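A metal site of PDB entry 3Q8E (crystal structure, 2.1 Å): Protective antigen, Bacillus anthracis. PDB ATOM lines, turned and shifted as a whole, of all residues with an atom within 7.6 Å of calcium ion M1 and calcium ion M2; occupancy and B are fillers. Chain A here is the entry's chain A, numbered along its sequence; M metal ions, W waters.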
ATOM      1  N   TYR A  22     -13.280   7.862 -26.384  1.00  0.00           N
ATOM      2  CA  TYR A  22     -13.205   8.741 -27.529  1.00  0.00           C
ATOM      3  C   TYR A  22     -12.347   8.042 -28.570  1.00  0.00           C
ATOM      4  O   TYR A  22     -11.187   7.783 -28.340  1.00  0.00           O
ATOM      5  CB  TYR A  22     -12.579  10.089 -27.148  1.00  0.00           C
ATOM      6  CG  TYR A  22     -13.397  10.827 -26.102  1.00  0.00           C
ATOM      7  CD1 TYR A  22     -12.987  10.899 -24.783  1.00  0.00           C
ATOM      8  CD2 TYR A  22     -14.599  11.427 -26.440  1.00  0.00           C
ATOM      9  CE1 TYR A  22     -13.756  11.557 -23.835  1.00  0.00           C
ATOM     10  CE2 TYR A  22     -15.355  12.080 -25.519  1.00  0.00           C
ATOM     11  CZ  TYR A  22     -14.942  12.157 -24.222  1.00  0.00           C
ATOM     12  OH  TYR A  22     -15.720  12.817 -23.335  1.00  0.00           O
ATOM     13  N   PRO A 176     -10.610  18.101 -25.865  1.00  0.00           N
ATOM     14  CA  PRO A 176     -11.217  19.382 -25.531  1.00  0.00           C
ATOM     15  C   PRO A 176     -12.722  19.249 -25.230  1.00  0.00           C
ATOM     16  O   PRO A 176     -13.489  18.772 -26.059  1.00  0.00           O
ATOM     17  CB  PRO A 176     -10.964  20.235 -26.785  1.00  0.00           C
ATOM     18  CG  PRO A 176     -10.022  19.392 -27.669  1.00  0.00           C
ATOM     19  CD  PRO A 176     -10.323  17.969 -27.293  1.00  0.00           C
ATOM     20  N   ASP A 177     -13.068  19.651 -24.016  1.00  0.00           N
ATOM     21  CA  ASP A 177     -14.399  19.513 -23.441  1.00  0.00           C
ATOM     22  C   ASP A 177     -14.557  20.631 -22.411  1.00  0.00           C
ATOM     23  O   ASP A 177     -14.529  20.386 -21.212  1.00  0.00           O
ATOM     24  CB  ASP A 177     -14.556  18.141 -22.770  1.00  0.00           C
ATOM     25  CG  ASP A 177     -16.009  17.882 -22.308  1.00  0.00           C
ATOM     26  OD1 ASP A 177     -16.906  18.654 -22.671  1.00  0.00           O
ATOM     27  OD2 ASP A 177     -16.265  16.907 -21.585  1.00  0.00           O
ATOM     28  N   ARG A 178     -14.703  21.864 -22.879  1.00  0.00           N
ATOM     29  CA  ARG A 178     -14.656  23.040 -22.015  1.00  0.00           C
ATOM     30  C   ARG A 178     -15.750  23.061 -20.927  1.00  0.00           C
ATOM     31  O   ARG A 178     -15.547  23.625 -19.866  1.00  0.00           O
ATOM     32  CB  ARG A 178     -14.760  24.314 -22.865  1.00  0.00           C
ATOM     33  CG  ARG A 178     -13.677  24.436 -23.952  1.00  0.00           C
ATOM     34  CD  ARG A 178     -14.055  25.383 -25.111  1.00  0.00           C
ATOM     35  NE  ARG A 178     -13.701  26.773 -24.844  1.00  0.00           N
ATOM     36  CZ  ARG A 178     -12.458  27.217 -24.701  1.00  0.00           C
ATOM     37  NH1 ARG A 178     -11.433  26.376 -24.773  1.00  0.00           N
ATOM     38  NH2 ARG A 178     -12.233  28.509 -24.465  1.00  0.00           N
ATOM     39  N   ASP A 179     -16.925  22.488 -21.185  1.00  0.00           N
ATOM     40  CA  ASP A 179     -18.007  22.521 -20.153  1.00  0.00           C
ATOM     41  C   ASP A 179     -18.117  21.212 -19.388  1.00  0.00           C
ATOM     42  O   ASP A 179     -19.006  21.036 -18.562  1.00  0.00           O
ATOM     43  CB  ASP A 179     -19.365  22.815 -20.793  1.00  0.00           C
ATOM     44  CG  ASP A 179     -19.649  21.879 -21.936  1.00  0.00           C
ATOM     45  OD1 ASP A 179     -19.155  20.739 -21.933  1.00  0.00           O
ATOM     46  OD2 ASP A 179     -20.334  22.296 -22.876  1.00  0.00           O
ATOM     47  N   ASN A 180     -17.233  20.275 -19.691  1.00  0.00           N
ATOM     48  CA  ASN A 180     -17.216  18.996 -19.016  1.00  0.00           C
ATOM     49  C   ASN A 180     -18.523  18.194 -19.116  1.00  0.00           C
ATOM     50  O   ASN A 180     -18.858  17.460 -18.186  1.00  0.00           O
ATOM     51  CB  ASN A 180     -16.849  19.188 -17.539  1.00  0.00           C
ATOM     52  CG  ASN A 180     -16.289  17.925 -16.906  1.00  0.00           C
ATOM     53  OD1 ASN A 180     -15.505  17.217 -17.525  1.00  0.00           O
ATOM     54  ND2 ASN A 180     -16.716  17.601 -15.698  1.00  0.00           N
ATOM     55  N   ASP A 181     -19.286  18.306 -20.211  1.00  0.00           N
ATOM     56  CA  ASP A 181     -20.472  17.447 -20.277  1.00  0.00           C
ATOM     57  C   ASP A 181     -20.097  16.092 -20.860  1.00  0.00           C
ATOM     58  O   ASP A 181     -20.836  15.119 -20.747  1.00  0.00           O
ATOM     59  CB  ASP A 181     -21.676  18.098 -21.002  1.00  0.00           C
ATOM     60  CG  ASP A 181     -21.339  18.590 -22.381  1.00  0.00           C
ATOM     61  OD1 ASP A 181     -20.424  18.030 -23.015  1.00  0.00           O
ATOM     62  OD2 ASP A 181     -21.991  19.535 -22.824  1.00  0.00           O
ATOM     63  N   GLY A 182     -18.896  16.005 -21.438  1.00  0.00           N
ATOM     64  CA  GLY A 182     -18.453  14.769 -22.040  1.00  0.00           C
ATOM     65  C   GLY A 182     -18.493  14.746 -23.571  1.00  0.00           C
ATOM     66  O   GLY A 182     -17.956  13.842 -24.190  1.00  0.00           O
ATOM     67  N   ILE A 183     -19.164  15.710 -24.197  1.00  0.00           N
ATOM     68  CA  ILE A 183     -19.189  15.795 -25.656  1.00  0.00           C
ATOM     69  C   ILE A 183     -18.099  16.781 -26.047  1.00  0.00           C
ATOM     70  O   ILE A 183     -18.126  17.910 -25.587  1.00  0.00           O
ATOM     71  CB  ILE A 183     -20.532  16.332 -26.186  1.00  0.00           C
ATOM     72  CG1 ILE A 183     -21.709  15.495 -25.637  1.00  0.00           C
ATOM     73  CG2 ILE A 183     -20.493  16.343 -27.726  1.00  0.00           C
ATOM     74  CD1 ILE A 183     -23.062  16.017 -26.004  1.00  0.00           C
ATOM     75  N   PRO A 184     -17.134  16.368 -26.882  1.00  0.00           N
ATOM     76  CA  PRO A 184     -16.010  17.217 -27.303  1.00  0.00           C
ATOM     77  C   PRO A 184     -16.460  18.521 -27.976  1.00  0.00           C
ATOM     78  O   PRO A 184     -17.467  18.505 -28.681  1.00  0.00           O
ATOM     79  CB  PRO A 184     -15.251  16.326 -28.307  1.00  0.00           C
ATOM     80  CG  PRO A 184     -15.590  14.929 -27.913  1.00  0.00           C
ATOM     81  CD  PRO A 184     -17.000  14.980 -27.368  1.00  0.00           C
ATOM     82  N   ASP A 185     -15.759  19.625 -27.747  1.00  0.00           N
ATOM     83  CA  ASP A 185     -16.187  20.925 -28.256  1.00  0.00           C
ATOM     84  C   ASP A 185     -16.583  20.855 -29.729  1.00  0.00           C
ATOM     85  O   ASP A 185     -17.589  21.453 -30.145  1.00  0.00           O
ATOM     86  CB  ASP A 185     -15.086  21.968 -28.144  1.00  0.00           C
ATOM     87  CG  ASP A 185     -14.554  22.147 -26.747  1.00  0.00           C
ATOM     88  OD1 ASP A 185     -15.177  21.664 -25.764  1.00  0.00           O
ATOM     89  OD2 ASP A 185     -13.470  22.779 -26.629  1.00  0.00           O
ATOM     90  N   SER A 186     -15.780  20.153 -30.515  1.00  0.00           N
ATOM     91  CA  SER A 186     -15.887  20.217 -31.973  1.00  0.00           C
ATOM     92  C   SER A 186     -17.120  19.502 -32.478  1.00  0.00           C
ATOM     93  O   SER A 186     -17.711  19.913 -33.483  1.00  0.00           O
ATOM     94  CB  SER A 186     -14.617  19.631 -32.657  1.00  0.00           C
ATOM     95  OG  SER A 186     -14.456  18.254 -32.374  1.00  0.00           O
ATOM     96  N   GLU A 188     -19.906  19.286 -30.616  1.00  0.00           N
ATOM     97  CA  GLU A 188     -21.021  20.145 -30.198  1.00  0.00           C
ATOM     98  C   GLU A 188     -21.209  21.311 -31.172  1.00  0.00           C
ATOM     99  O   GLU A 188     -22.332  21.741 -31.475  1.00  0.00           O
ATOM    100  CB  GLU A 188     -20.768  20.687 -28.792  1.00  0.00           C
ATOM    101  CG  GLU A 188     -20.888  19.635 -27.700  1.00  0.00           C
ATOM    102  CD  GLU A 188     -21.215  20.249 -26.374  1.00  0.00           C
ATOM    103  OE1 GLU A 188     -20.284  20.497 -25.616  1.00  0.00           O
ATOM    104  OE2 GLU A 188     -22.408  20.530 -26.081  1.00  0.00           O
ATOM    105  N   TYR A 192     -23.717  16.636 -34.330  1.00  0.00           N
ATOM    106  CA  TYR A 192     -23.566  15.232 -34.018  1.00  0.00           C
ATOM    107  C   TYR A 192     -24.895  14.496 -34.043  1.00  0.00           C
ATOM    108  O   TYR A 192     -25.974  15.098 -34.002  1.00  0.00           O
ATOM    109  CB  TYR A 192     -22.919  15.051 -32.650  1.00  0.00           C
ATOM    110  CG  TYR A 192     -23.604  15.732 -31.468  1.00  0.00           C
ATOM    111  CD1 TYR A 192     -23.443  17.088 -31.250  1.00  0.00           C
ATOM    112  CD2 TYR A 192     -24.366  14.996 -30.554  1.00  0.00           C
ATOM    113  CE1 TYR A 192     -24.060  17.719 -30.165  1.00  0.00           C
ATOM    114  CE2 TYR A 192     -24.993  15.626 -29.466  1.00  0.00           C
ATOM    115  CZ  TYR A 192     -24.823  16.990 -29.283  1.00  0.00           C
ATOM    116  OH  TYR A 192     -25.405  17.636 -28.217  1.00  0.00           O
ATOM    117  N   SER A 221     -25.004  21.908 -30.014  1.00  0.00           N
ATOM    118  CA  SER A 221     -25.095  22.402 -28.641  1.00  0.00           C
ATOM    119  C   SER A 221     -23.911  23.316 -28.304  1.00  0.00           C
ATOM    120  O   SER A 221     -22.936  23.375 -29.055  1.00  0.00           O
ATOM    121  CB  SER A 221     -25.243  21.231 -27.662  1.00  0.00           C
ATOM    122  OG  SER A 221     -24.372  20.147 -27.948  1.00  0.00           O
ATOM    123  N   SER A 222     -24.018  24.089 -27.234  1.00  0.00           N
ATOM    124  CA  SER A 222     -22.887  24.951 -26.847  1.00  0.00           C
ATOM    125  C   SER A 222     -21.798  24.153 -26.157  1.00  0.00           C
ATOM    126  O   SER A 222     -22.078  23.469 -25.171  1.00  0.00           O
ATOM    127  CB  SER A 222     -23.307  26.049 -25.883  1.00  0.00           C
ATOM    128  OG  SER A 222     -22.140  26.707 -25.400  1.00  0.00           O
ATOM    129  N   PRO A 223     -20.546  24.283 -26.653  1.00  0.00           N
ATOM    130  CA  PRO A 223     -19.367  23.606 -26.043  1.00  0.00           C
ATOM    131  C   PRO A 223     -18.966  24.227 -24.715  1.00  0.00           C
ATOM    132  O   PRO A 223     -18.108  23.672 -24.024  1.00  0.00           O
ATOM    133  CB  PRO A 223     -18.253  23.829 -27.075  1.00  0.00           C
ATOM    134  CG  PRO A 223     -18.596  25.132 -27.742  1.00  0.00           C
ATOM    135  CD  PRO A 223     -20.165  25.188 -27.756  1.00  0.00           C
ATOM    136  N   GLU A 224     -19.584  25.340 -24.358  1.00  0.00           N
ATOM    137  CA  GLU A 224     -19.336  26.061 -23.118  1.00  0.00           C
ATOM    138  C   GLU A 224     -20.493  26.036 -22.105  1.00  0.00           C
ATOM    139  O   GLU A 224     -20.396  26.673 -21.058  1.00  0.00           O
ATOM    140  CB  GLU A 224     -19.039  27.499 -23.468  1.00  0.00           C
ATOM    141  CG  GLU A 224     -18.088  27.584 -24.679  1.00  0.00           C
ATOM    142  CD  GLU A 224     -16.949  28.561 -24.496  1.00  0.00           C
ATOM    143  OE1 GLU A 224     -15.949  28.473 -25.275  1.00  0.00           O
ATOM    144  OE2 GLU A 224     -17.053  29.421 -23.592  1.00  0.00           O
ATOM    145  N   LYS A 225     -21.588  25.356 -22.435  1.00  0.00           N
ATOM    146  CA  LYS A 225     -22.708  25.177 -21.510  1.00  0.00           C
ATOM    147  C   LYS A 225     -22.922  23.695 -21.240  1.00  0.00           C
ATOM    148  O   LYS A 225     -23.310  22.941 -22.138  1.00  0.00           O
ATOM    149  CB  LYS A 225     -23.953  25.787 -22.143  1.00  0.00           C
ATOM    150  CG  LYS A 225     -23.808  27.278 -22.365  1.00  0.00           C
ATOM    151  CD  LYS A 225     -25.169  27.944 -22.689  1.00  0.00           C
ATOM    152  CE  LYS A 225     -25.872  28.328 -21.411  1.00  0.00           C
ATOM    153  NZ  LYS A 225     -27.295  28.394 -21.656  1.00  0.00           N
ATOM    154  N   TRP A 226     -22.658  23.263 -20.009  1.00  0.00           N
ATOM    155  CA  TRP A 226     -22.887  21.880 -19.628  1.00  0.00           C
ATOM    156  C   TRP A 226     -24.342  21.480 -19.992  1.00  0.00           C
ATOM    157  O   TRP A 226     -24.553  20.427 -20.581  1.00  0.00           O
ATOM    158  CB  TRP A 226     -22.566  21.727 -18.122  1.00  0.00           C
ATOM    159  CG  TRP A 226     -22.815  20.411 -17.526  1.00  0.00           C
ATOM    160  CD1 TRP A 226     -21.950  19.374 -17.455  1.00  0.00           C
ATOM    161  CD2 TRP A 226     -24.011  19.993 -16.829  1.00  0.00           C
ATOM    162  NE1 TRP A 226     -22.521  18.323 -16.780  1.00  0.00           N
ATOM    163  CE2 TRP A 226     -23.794  18.675 -16.392  1.00  0.00           C
ATOM    164  CE3 TRP A 226     -25.252  20.598 -16.571  1.00  0.00           C
ATOM    165  CZ2 TRP A 226     -24.749  17.940 -15.682  1.00  0.00           C
ATOM    166  CZ3 TRP A 226     -26.219  19.864 -15.868  1.00  0.00           C
ATOM    167  CH2 TRP A 226     -25.959  18.545 -15.424  1.00  0.00           C
ATOM    168  N   SER A 227     -25.314  22.334 -19.687  1.00  0.00           N
ATOM    169  CA  SER A 227     -26.678  22.203 -20.252  1.00  0.00           C
ATOM    170  C   SER A 227     -26.904  23.411 -21.139  1.00  0.00           C
ATOM    171  O   SER A 227     -26.928  24.557 -20.666  1.00  0.00           O
ATOM    172  CB  SER A 227     -27.752  22.150 -19.154  1.00  0.00           C
ATOM    173  OG  SER A 227     -29.066  22.154 -19.729  1.00  0.00           O
ATOM    174  N   THR A 228     -27.063  23.184 -22.436  1.00  0.00           N
ATOM    175  CA  THR A 228     -27.168  24.281 -23.366  1.00  0.00           C
ATOM    176  C   THR A 228     -28.483  25.044 -23.136  1.00  0.00           C
ATOM    177  O   THR A 228     -28.538  26.263 -23.294  1.00  0.00           O
ATOM    178  CB  THR A 228     -27.000  23.770 -24.800  1.00  0.00           C
ATOM    179  OG1 THR A 228     -25.641  23.333 -24.977  1.00  0.00           O
ATOM    180  CG2 THR A 228     -27.323  24.911 -25.809  1.00  0.00           C
ATOM    181  N   SER A 234     -27.457  17.510 -18.426  1.00  0.00           N
ATOM    182  CA  SER A 234     -26.362  17.905 -19.308  1.00  0.00           C
ATOM    183  C   SER A 234     -26.692  17.494 -20.757  1.00  0.00           C
ATOM    184  O   SER A 234     -27.483  16.563 -20.994  1.00  0.00           O
ATOM    185  CB  SER A 234     -25.055  17.239 -18.890  1.00  0.00           C
ATOM    186  OG  SER A 234     -24.844  16.061 -19.639  1.00  0.00           O
ATOM    187  N   ASP A 235     -26.039  18.143 -21.705  1.00  0.00           N
ATOM    188  CA  ASP A 235     -26.275  17.850 -23.128  1.00  0.00           C
ATOM    189  C   ASP A 235     -25.986  16.391 -23.413  1.00  0.00           C
ATOM    190  O   ASP A 235     -26.697  15.748 -24.177  1.00  0.00           O
ATOM    191  CB  ASP A 235     -25.407  18.752 -24.000  1.00  0.00           C
ATOM    192  CG  ASP A 235     -25.750  20.212 -23.815  1.00  0.00           C
ATOM    193  OD1 ASP A 235     -26.890  20.522 -23.416  1.00  0.00           O
ATOM    194  OD2 ASP A 235     -24.915  21.066 -24.083  1.00  0.00           O
ATOM    195  N   PHE A 236     -24.950  15.865 -22.755  1.00  0.00           N
ATOM    196  CA  PHE A 236     -24.601  14.444 -22.880  1.00  0.00           C
ATOM    197  C   PHE A 236     -25.655  13.529 -22.196  1.00  0.00           C
ATOM    198  O   PHE A 236     -26.066  12.515 -22.741  1.00  0.00           O
ATOM    199  CB  PHE A 236     -23.215  14.234 -22.297  1.00  0.00           C
ATOM    200  CG  PHE A 236     -22.684  12.842 -22.403  1.00  0.00           C
ATOM    201  CD1 PHE A 236     -22.194  12.360 -23.617  1.00  0.00           C
ATOM    202  CD2 PHE A 236     -22.611  12.029 -21.273  1.00  0.00           C
ATOM    203  CE1 PHE A 236     -21.660  11.070 -23.724  1.00  0.00           C
ATOM    204  CE2 PHE A 236     -22.071  10.736 -21.360  1.00  0.00           C
ATOM    205  CZ  PHE A 236     -21.597  10.257 -22.591  1.00  0.00           C
ATOM    206  N   PRO A 254     -30.770  18.747 -26.634  1.00  0.00           N
ATOM    207  CA  PRO A 254     -29.967  19.724 -25.895  1.00  0.00           C
ATOM    208  C   PRO A 254     -30.496  21.161 -25.997  1.00  0.00           C
ATOM    209  O   PRO A 254     -30.248  21.963 -25.095  1.00  0.00           O
ATOM    210  CB  PRO A 254     -28.582  19.600 -26.532  1.00  0.00           C
ATOM    211  CG  PRO A 254     -28.527  18.225 -27.032  1.00  0.00           C
ATOM    212  CD  PRO A 254     -29.933  17.885 -27.486  1.00  0.00           C
HETATM  213 CA    CA M   1     -22.437  21.450 -23.920  1.00  0.00          CA
HETATM  214 CA    CA M   2     -18.803  19.501 -24.023  1.00  0.00          CA
HETATM  215  O   HOH W   1     -17.425  21.351 -24.709  1.00  0.00           O
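OG1 of Thr 228 touches calcium ion M1, at 3.9 Å. Seven residues have an atom within 4 Å of calcium ion M1: Asp 179, Asp 181, Glu 188, Ser 222, Lys 225, Thr 228 and Asp 235. The nearest printed residue that does not touch calcium ion M1 is Trp 226 (4.1 Å).
Calcium ion M2 is bound by O of Ile 183, OE1 of Glu 188, water W1, OD1 of Asp 181, OD1 of Asp 179 and OD1 of Asp 177.
OD2 of Asp 177 is in hydrogen-bond range of N of Gly 182 (2.8 Å). The backbone carbonyl oxygen of Thr 228 is in hydrogen-bond range of the side-chain amino group of Lys 225 (3.0 Å). The side-chain carboxylate (OD2) of Asp 179 sits close to the backbone NH (N) of Glu 224. The backbone NH (N) of Lys 225 lies within hydrogen-bond range of the side-chain hydroxyl (OG) of Ser 222. The backbone NH (N) of Glu 224 sits at hydrogen-bond distance from the side-chain hydroxyl (OG) of Ser 222. The backbone NH (N) of Thr 228 is in hydrogen-bond range of the side-chain carboxylate (OD1) of Asp 235 (2.8 Å). The side-chain carboxylate of Asp 177 lies close to the backbone NH of Asn 180, at 3.4 Å. The backbone NH (N) of Asp 177 lies close to the side-chain carboxylate (OD1) of Asp 185 (3.4 Å).
The nearest printed residue that does not touch calcium ion M2 is Pro 223 (4.2 Å).
Calcium ion M1 is bound by the side-chain carboxylate of Asp 181 (2.3 Å), the side-chain carboxylate of Glu 188 (2.3 Å), the backbone carbonyl oxygen of Ser 222 (2.4 Å), the backbone carbonyl oxygen of Lys 225 (2.5 Å), the side-chain carboxylate of Asp 179 (2.5 Å) and the side-chain carboxylate of Asp 235 (2.5 Å). Slightly farther from calcium ion M1 lies the side-chain carboxylate (OE1) of Glu 188 (2.9 Å).
Water W1 lies within hydrogen-bond range of OD1 of Asp 185 (2.5 Å), O of Pro 223 (2.5 Å) and N of Arg 178 (3.3 Å).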
